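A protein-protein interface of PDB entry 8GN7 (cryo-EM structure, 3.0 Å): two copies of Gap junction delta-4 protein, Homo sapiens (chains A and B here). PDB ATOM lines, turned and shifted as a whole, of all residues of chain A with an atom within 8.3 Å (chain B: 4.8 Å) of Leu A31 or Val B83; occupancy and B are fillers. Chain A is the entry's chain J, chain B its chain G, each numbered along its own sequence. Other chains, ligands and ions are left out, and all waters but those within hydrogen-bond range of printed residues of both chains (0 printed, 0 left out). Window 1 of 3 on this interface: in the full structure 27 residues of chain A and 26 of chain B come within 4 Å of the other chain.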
ATOM      1  N   TRP A  25      13.521  15.693  25.728  1.00  0.00           N
ATOM      2  CA  TRP A  25      12.075  15.683  25.923  1.00  0.00           C
ATOM      3  C   TRP A  25      11.343  16.043  24.638  1.00  0.00           C
ATOM      4  O   TRP A  25      10.328  15.422  24.301  1.00  0.00           O
ATOM      5  CB  TRP A  25      11.696  16.653  27.045  1.00  0.00           C
ATOM      6  CG  TRP A  25      10.217  16.906  27.205  1.00  0.00           C
ATOM      7  CD1 TRP A  25       9.365  16.257  28.048  1.00  0.00           C
ATOM      8  CD2 TRP A  25       9.430  17.892  26.522  1.00  0.00           C
ATOM      9  NE1 TRP A  25       8.096  16.767  27.926  1.00  0.00           N
ATOM     10  CE2 TRP A  25       8.110  17.773  26.996  1.00  0.00           C
ATOM     11  CE3 TRP A  25       9.714  18.860  25.554  1.00  0.00           C
ATOM     12  CZ2 TRP A  25       7.075  18.582  26.532  1.00  0.00           C
ATOM     13  CZ3 TRP A  25       8.685  19.662  25.094  1.00  0.00           C
ATOM     14  CH2 TRP A  25       7.383  19.517  25.583  1.00  0.00           C
ATOM     15  N   PHE A  26      11.846  17.043  23.913  1.00  0.00           N
ATOM     16  CA  PHE A  26      11.232  17.440  22.652  1.00  0.00           C
ATOM     17  C   PHE A  26      11.235  16.290  21.655  1.00  0.00           C
ATOM     18  O   PHE A  26      10.244  16.067  20.951  1.00  0.00           O
ATOM     19  CB  PHE A  26      11.969  18.650  22.083  1.00  0.00           C
ATOM     20  CG  PHE A  26      11.362  19.203  20.829  1.00  0.00           C
ATOM     21  CD1 PHE A  26      10.220  19.981  20.880  1.00  0.00           C
ATOM     22  CD2 PHE A  26      11.941  18.951  19.597  1.00  0.00           C
ATOM     23  CE1 PHE A  26       9.668  20.497  19.726  1.00  0.00           C
ATOM     24  CE2 PHE A  26      11.391  19.462  18.440  1.00  0.00           C
ATOM     25  CZ  PHE A  26      10.253  20.235  18.504  1.00  0.00           C
ATOM     26  N   VAL A  27      12.341  15.547  21.585  1.00  0.00           N
ATOM     27  CA  VAL A  27      12.420  14.418  20.665  1.00  0.00           C
ATOM     28  C   VAL A  27      11.459  13.313  21.084  1.00  0.00           C
ATOM     29  O   VAL A  27      10.730  12.762  20.249  1.00  0.00           O
ATOM     30  CB  VAL A  27      13.871  13.911  20.573  1.00  0.00           C
ATOM     31  CG1 VAL A  27      13.905  12.472  20.085  1.00  0.00           C
ATOM     32  CG2 VAL A  27      14.683  14.808  19.652  1.00  0.00           C
ATOM     33  N   LEU A  28      11.432  12.972  22.375  1.00  0.00           N
ATOM     34  CA  LEU A  28      10.610  11.844  22.812  1.00  0.00           C
ATOM     35  C   LEU A  28       9.118  12.141  22.691  1.00  0.00           C
ATOM     36  O   LEU A  28       8.367  11.346  22.115  1.00  0.00           O
ATOM     37  CB  LEU A  28      10.961  11.432  24.241  1.00  0.00           C
ATOM     38  CG  LEU A  28      12.078  10.394  24.343  1.00  0.00           C
ATOM     39  CD1 LEU A  28      12.898  10.592  25.593  1.00  0.00           C
ATOM     40  CD2 LEU A  28      11.495   8.988  24.292  1.00  0.00           C
ATOM     41  N   THR A  29       8.659  13.274  23.227  1.00  0.00           N
ATOM     42  CA  THR A  29       7.212  13.509  23.244  1.00  0.00           C
ATOM     43  C   THR A  29       6.711  14.210  21.984  1.00  0.00           C
ATOM     44  O   THR A  29       5.821  15.064  22.022  1.00  0.00           O
ATOM     45  CB  THR A  29       6.837  14.293  24.503  1.00  0.00           C
ATOM     46  OG1 THR A  29       5.421  14.223  24.714  1.00  0.00           O
ATOM     47  CG2 THR A  29       7.277  15.759  24.425  1.00  0.00           C
ATOM     48  N   MET A  30       7.213  13.792  20.825  1.00  0.00           N
ATOM     49  CA  MET A  30       6.562  14.065  19.548  1.00  0.00           C
ATOM     50  C   MET A  30       6.641  12.896  18.581  1.00  0.00           C
ATOM     51  O   MET A  30       5.838  12.836  17.644  1.00  0.00           O
ATOM     52  CB  MET A  30       7.154  15.323  18.892  1.00  0.00           C
ATOM     53  CG  MET A  30       6.453  15.770  17.609  1.00  0.00           C
ATOM     54  SD  MET A  30       6.139  17.541  17.530  1.00  0.00           S
ATOM     55  CE  MET A  30       7.500  18.140  18.509  1.00  0.00           C
ATOM     56  N   LEU A  31       7.537  11.937  18.802  1.00  0.00           N
ATOM     57  CA  LEU A  31       7.642  10.736  17.989  1.00  0.00           C
ATOM     58  C   LEU A  31       6.906   9.553  18.597  1.00  0.00           C
ATOM     59  O   LEU A  31       6.468   8.662  17.862  1.00  0.00           O
ATOM     60  CB  LEU A  31       9.117  10.369  17.795  1.00  0.00           C
ATOM     61  CG  LEU A  31       9.471   9.297  16.769  1.00  0.00           C
ATOM     62  CD1 LEU A  31       9.785   9.937  15.430  1.00  0.00           C
ATOM     63  CD2 LEU A  31      10.647   8.478  17.258  1.00  0.00           C
ATOM     64  N   LEU A  32       6.759   9.531  19.919  1.00  0.00           N
ATOM     65  CA  LEU A  32       6.033   8.479  20.613  1.00  0.00           C
ATOM     66  C   LEU A  32       4.700   8.953  21.171  1.00  0.00           C
ATOM     67  O   LEU A  32       3.925   8.130  21.667  1.00  0.00           O
ATOM     68  CB  LEU A  32       6.889   7.906  21.747  1.00  0.00           C
ATOM     69  CG  LEU A  32       7.939   6.863  21.358  1.00  0.00           C
ATOM     70  CD1 LEU A  32       8.945   6.676  22.479  1.00  0.00           C
ATOM     71  CD2 LEU A  32       7.273   5.547  21.003  1.00  0.00           C
ATOM     72  N   ARG A  33       4.415  10.251  21.115  1.00  0.00           N
ATOM     73  CA  ARG A  33       3.166  10.793  21.634  1.00  0.00           C
ATOM     74  C   ARG A  33       2.308  11.425  20.551  1.00  0.00           C
ATOM     75  O   ARG A  33       1.138  11.059  20.404  1.00  0.00           O
ATOM     76  CB  ARG A  33       3.460  11.821  22.737  1.00  0.00           C
ATOM     77  CG  ARG A  33       2.223  12.374  23.421  1.00  0.00           C
ATOM     78  CD  ARG A  33       2.473  12.578  24.905  1.00  0.00           C
ATOM     79  NE  ARG A  33       1.326  13.168  25.584  1.00  0.00           N
ATOM     80  CZ  ARG A  33       1.412  14.072  26.550  1.00  0.00           C
ATOM     81  NH1 ARG A  33       2.581  14.528  26.967  1.00  0.00           N
ATOM     82  NH2 ARG A  33       0.298  14.530  27.111  1.00  0.00           N
ATOM     83  N   MET A  34       2.858  12.363  19.785  1.00  0.00           N
ATOM     84  CA  MET A  34       2.107  13.043  18.739  1.00  0.00           C
ATOM     85  C   MET A  34       1.972  12.220  17.467  1.00  0.00           C
ATOM     86  O   MET A  34       1.136  12.552  16.621  1.00  0.00           O
ATOM     87  CB  MET A  34       2.762  14.388  18.408  1.00  0.00           C
ATOM     88  CG  MET A  34       2.325  15.526  19.312  1.00  0.00           C
ATOM     89  SD  MET A  34       0.644  16.068  18.952  1.00  0.00           S
ATOM     90  CE  MET A  34      -0.197  15.570  20.451  1.00  0.00           C
ATOM     91  N   LEU A  35       2.768  11.165  17.310  1.00  0.00           N
ATOM     92  CA  LEU A  35       2.688  10.305  16.137  1.00  0.00           C
ATOM     93  C   LEU A  35       1.793   9.094  16.346  1.00  0.00           C
ATOM     94  O   LEU A  35       1.068   8.708  15.425  1.00  0.00           O
ATOM     95  CB  LEU A  35       4.087   9.833  15.730  1.00  0.00           C
ATOM     96  CG  LEU A  35       4.356   9.720  14.230  1.00  0.00           C
ATOM     97  CD1 LEU A  35       4.146  11.061  13.549  1.00  0.00           C
ATOM     98  CD2 LEU A  35       5.761   9.201  13.975  1.00  0.00           C
ATOM     99  N   VAL A  36       1.830   8.486  17.533  1.00  0.00           N
ATOM    100  CA  VAL A  36       0.943   7.364  17.825  1.00  0.00           C
ATOM    101  C   VAL A  36      -0.508   7.821  17.876  1.00  0.00           C
ATOM    102  O   VAL A  36      -1.412   7.081  17.471  1.00  0.00           O
ATOM    103  CB  VAL A  36       1.368   6.682  19.138  1.00  0.00           C
ATOM    104  CG1 VAL A  36       0.588   5.397  19.347  1.00  0.00           C
ATOM    105  CG2 VAL A  36       2.859   6.402  19.123  1.00  0.00           C
ATOM    106  N   ILE A  37      -0.759   9.032  18.371  1.00  0.00           N
ATOM    107  CA  ILE A  37      -2.124   9.545  18.432  1.00  0.00           C
ATOM    108  C   ILE A  37      -2.698   9.713  17.031  1.00  0.00           C
ATOM    109  O   ILE A  37      -3.855   9.362  16.773  1.00  0.00           O
ATOM    110  CB  ILE A  37      -2.156  10.865  19.225  1.00  0.00           C
ATOM    111  CG1 ILE A  37      -2.176  10.587  20.727  1.00  0.00           C
ATOM    112  CG2 ILE A  37      -3.356  11.709  18.829  1.00  0.00           C
ATOM    113  CD1 ILE A  37      -1.948  11.816  21.571  1.00  0.00           C
ATOM    114  N   LEU A  39      -1.343   8.534  13.817  1.00  0.00           N
ATOM    115  CA  LEU A  39      -1.266   7.378  12.933  1.00  0.00           C
ATOM    116  C   LEU A  39      -1.952   6.139  13.490  1.00  0.00           C
ATOM    117  O   LEU A  39      -2.541   5.373  12.720  1.00  0.00           O
ATOM    118  CB  LEU A  39       0.196   7.048  12.623  1.00  0.00           C
ATOM    119  CG  LEU A  39       0.962   8.073  11.785  1.00  0.00           C
ATOM    120  CD1 LEU A  39       2.403   7.635  11.592  1.00  0.00           C
ATOM    121  CD2 LEU A  39       0.281   8.282  10.444  1.00  0.00           C
ATOM    122  N   ALA A  40      -1.893   5.915  14.803  1.00  0.00           N
ATOM    123  CA  ALA A  40      -2.437   4.703  15.397  1.00  0.00           C
ATOM    124  C   ALA A  40      -3.706   4.929  16.206  1.00  0.00           C
ATOM    125  O   ALA A  40      -4.371   3.951  16.561  1.00  0.00           O
ATOM    126  CB  ALA A  40      -1.386   4.029  16.292  1.00  0.00           C
ATOM    127  N   PHE A 200      -0.387   2.416  27.223  1.00  0.00           N
ATOM    128  CA  PHE A 200       0.799   2.938  26.551  1.00  0.00           C
ATOM    129  C   PHE A 200       0.858   4.458  26.643  1.00  0.00           C
ATOM    130  O   PHE A 200       1.902   5.026  26.997  1.00  0.00           O
ATOM    131  CB  PHE A 200       0.806   2.477  25.093  1.00  0.00           C
ATOM    132  CG  PHE A 200       1.964   2.997  24.286  1.00  0.00           C
ATOM    133  CD1 PHE A 200       3.175   2.328  24.276  1.00  0.00           C
ATOM    134  CD2 PHE A 200       1.834   4.137  23.511  1.00  0.00           C
ATOM    135  CE1 PHE A 200       4.238   2.795  23.530  1.00  0.00           C
ATOM    136  CE2 PHE A 200       2.894   4.608  22.763  1.00  0.00           C
ATOM    137  CZ  PHE A 200       4.096   3.936  22.772  1.00  0.00           C
ATOM    138  N   VAL A 204       3.551   6.832  28.661  1.00  0.00           N
ATOM    139  CA  VAL A 204       4.300   7.877  27.967  1.00  0.00           C
ATOM    140  C   VAL A 204       4.126   9.219  28.671  1.00  0.00           C
ATOM    141  O   VAL A 204       5.099   9.952  28.893  1.00  0.00           O
ATOM    142  CB  VAL A 204       3.871   7.951  26.491  1.00  0.00           C
ATOM    143  CG1 VAL A 204       4.254   9.292  25.889  1.00  0.00           C
ATOM    144  CG2 VAL A 204       4.496   6.814  25.705  1.00  0.00           C
ATOM    145  N   MET B  34       8.778   2.711   6.349  1.00  0.00           N
ATOM    146  CA  MET B  34       7.852   3.647   6.969  1.00  0.00           C
ATOM    147  C   MET B  34       6.844   4.228   5.988  1.00  0.00           C
ATOM    148  O   MET B  34       5.862   4.837   6.424  1.00  0.00           O
ATOM    149  CB  MET B  34       8.624   4.788   7.640  1.00  0.00           C
ATOM    150  CG  MET B  34       9.290   4.398   8.950  1.00  0.00           C
ATOM    151  SD  MET B  34       8.133   3.733  10.161  1.00  0.00           S
ATOM    152  CE  MET B  34       7.075   5.151  10.435  1.00  0.00           C
ATOM    153  N   LEU B  79       3.560  -0.432  13.273  1.00  0.00           N
ATOM    154  CA  LEU B  79       3.825   0.976  13.553  1.00  0.00           C
ATOM    155  C   LEU B  79       4.720   1.139  14.775  1.00  0.00           C
ATOM    156  O   LEU B  79       5.714   1.876  14.736  1.00  0.00           O
ATOM    157  CB  LEU B  79       2.509   1.726  13.754  1.00  0.00           C
ATOM    158  CG  LEU B  79       2.280   2.962  12.885  1.00  0.00           C
ATOM    159  CD1 LEU B  79       1.002   2.818  12.076  1.00  0.00           C
ATOM    160  CD2 LEU B  79       2.238   4.210  13.748  1.00  0.00           C
ATOM    161  N   ILE B  80       4.389   0.449  15.869  1.00  0.00           N
ATOM    162  CA  ILE B  80       5.157   0.601  17.102  1.00  0.00           C
ATOM    163  C   ILE B  80       6.569   0.055  16.927  1.00  0.00           C
ATOM    164  O   ILE B  80       7.539   0.639  17.425  1.00  0.00           O
ATOM    165  CB  ILE B  80       4.418  -0.069  18.277  1.00  0.00           C
ATOM    166  CG1 ILE B  80       3.617   0.969  19.067  1.00  0.00           C
ATOM    167  CG2 ILE B  80       5.387  -0.785  19.204  1.00  0.00           C
ATOM    168  CD1 ILE B  80       2.499   1.617  18.283  1.00  0.00           C
ATOM    169  N   GLN B  81       6.716  -1.066  16.214  1.00  0.00           N
ATOM    170  CA  GLN B  81       8.042  -1.635  16.004  1.00  0.00           C
ATOM    171  C   GLN B  81       8.900  -0.735  15.124  1.00  0.00           C
ATOM    172  O   GLN B  81      10.093  -0.559  15.389  1.00  0.00           O
ATOM    173  CB  GLN B  81       7.920  -3.034  15.401  1.00  0.00           C
ATOM    174  CG  GLN B  81       9.045  -3.415  14.458  1.00  0.00           C
ATOM    175  CD  GLN B  81       8.827  -4.766  13.812  1.00  0.00           C
ATOM    176  OE1 GLN B  81       7.695  -5.227  13.678  1.00  0.00           O
ATOM    177  NE2 GLN B  81       9.914  -5.413  13.414  1.00  0.00           N
ATOM    178  N   GLY B  82       8.314  -0.151  14.074  1.00  0.00           N
ATOM    179  CA  GLY B  82       9.074   0.741  13.218  1.00  0.00           C
ATOM    180  C   GLY B  82       9.418   2.073  13.844  1.00  0.00           C
ATOM    181  O   GLY B  82      10.472   2.635  13.533  1.00  0.00           O
ATOM    182  N   VAL B  83       8.557   2.591  14.717  1.00  0.00           N
ATOM    183  CA  VAL B  83       8.859   3.846  15.395  1.00  0.00           C
ATOM    184  C   VAL B  83       9.955   3.679  16.445  1.00  0.00           C
ATOM    185  O   VAL B  83      10.837   4.537  16.559  1.00  0.00           O
ATOM    186  CB  VAL B  83       7.581   4.431  16.018  1.00  0.00           C
ATOM    187  CG1 VAL B  83       7.919   5.498  17.045  1.00  0.00           C
ATOM    188  CG2 VAL B  83       6.681   5.001  14.936  1.00  0.00           C
ATOM    189  N   CYS B  84       9.936   2.582  17.201  1.00  0.00           N
ATOM    190  CA  CYS B  84      10.888   2.380  18.286  1.00  0.00           C
ATOM    191  C   CYS B  84      12.296   2.059  17.801  1.00  0.00           C
ATOM    192  O   CYS B  84      13.229   2.082  18.611  1.00  0.00           O
ATOM    193  CB  CYS B  84      10.398   1.263  19.209  1.00  0.00           C
ATOM    194  SG  CYS B  84       9.453   1.844  20.632  1.00  0.00           S
ATOM    195  N   VAL B  85      12.474   1.758  16.517  1.00  0.00           N
ATOM    196  CA  VAL B  85      13.809   1.521  15.980  1.00  0.00           C
ATOM    197  C   VAL B  85      14.458   2.820  15.506  1.00  0.00           C
ATOM    198  O   VAL B  85      15.682   2.970  15.593  1.00  0.00           O
ATOM    199  CB  VAL B  85      13.746   0.476  14.852  1.00  0.00           C
ATOM    200  CG1 VAL B  85      15.093   0.330  14.167  1.00  0.00           C
ATOM    201  CG2 VAL B  85      13.290  -0.863  15.403  1.00  0.00           C
ATOM    202  N   LEU B  86      13.664   3.775  15.025  1.00  0.00           N
ATOM    203  CA  LEU B  86      14.178   5.082  14.641  1.00  0.00           C
ATOM    204  C   LEU B  86      14.479   5.973  15.837  1.00  0.00           C
ATOM    205  O   LEU B  86      15.039   7.059  15.655  1.00  0.00           O
ATOM    206  CB  LEU B  86      13.181   5.790  13.721  1.00  0.00           C
ATOM    207  CG  LEU B  86      13.140   5.337  12.262  1.00  0.00           C
ATOM    208  CD1 LEU B  86      11.918   5.910  11.565  1.00  0.00           C
ATOM    209  CD2 LEU B  86      14.413   5.742  11.536  1.00  0.00           C
ATOM    210  N   LEU B  87      14.114   5.548  17.050  1.00  0.00           N
ATOM    211  CA  LEU B  87      14.343   6.390  18.224  1.00  0.00           C
ATOM    212  C   LEU B  87      15.816   6.475  18.607  1.00  0.00           C
ATOM    213  O   LEU B  87      16.289   7.588  18.898  1.00  0.00           O
ATOM    214  CB  LEU B  87      13.475   5.903  19.388  1.00  0.00           C
ATOM    215  CG  LEU B  87      13.534   6.713  20.682  1.00  0.00           C
ATOM    216  CD1 LEU B  87      12.513   7.837  20.654  1.00  0.00           C
ATOM    217  CD2 LEU B  87      13.305   5.810  21.880  1.00  0.00           C
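Printed residues of chain B that touch a printed residue of chain A: Leu B79, Val B83 and Leu B87.
Of the 17 printed residues of chain A, 3 touch a printed residue of chain B.
Hydrophobic or aromatic side chains of chain A within 4 Å of the printed part of chain B: Leu A28, Leu A31 and Leu A39.
Among the printed residues, no Asp or Glu carboxylate lies within 4 Å of a Lys or Arg side-chain nitrogen of the other chain.
Among the printed residues, pairs that only touch across the chains: Leu A28 with Leu B87, Leu A31 with Val B83, Leu A31 with Leu B87 and Leu A39 with Leu B79.
Position printed for both chains: 34.
Of the printed residues of chain B, Leu A31 touches Val B83 and Leu B87.
Printed residues of chain A within 4 Å of Val B83: Leu A31.
Printed residues of chain B within 4 Å of Leu A39: Leu B79 (3.7 Å).
Of the printed residues of chain A, Leu B79 touches Leu A39.
The nearest printed residue of chain B that does not touch Leu A31 is Leu B86 (4.8 Å).
The nearest printed residue of chain B that does not touch Leu A39 is Met B34 (5.4 Å).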
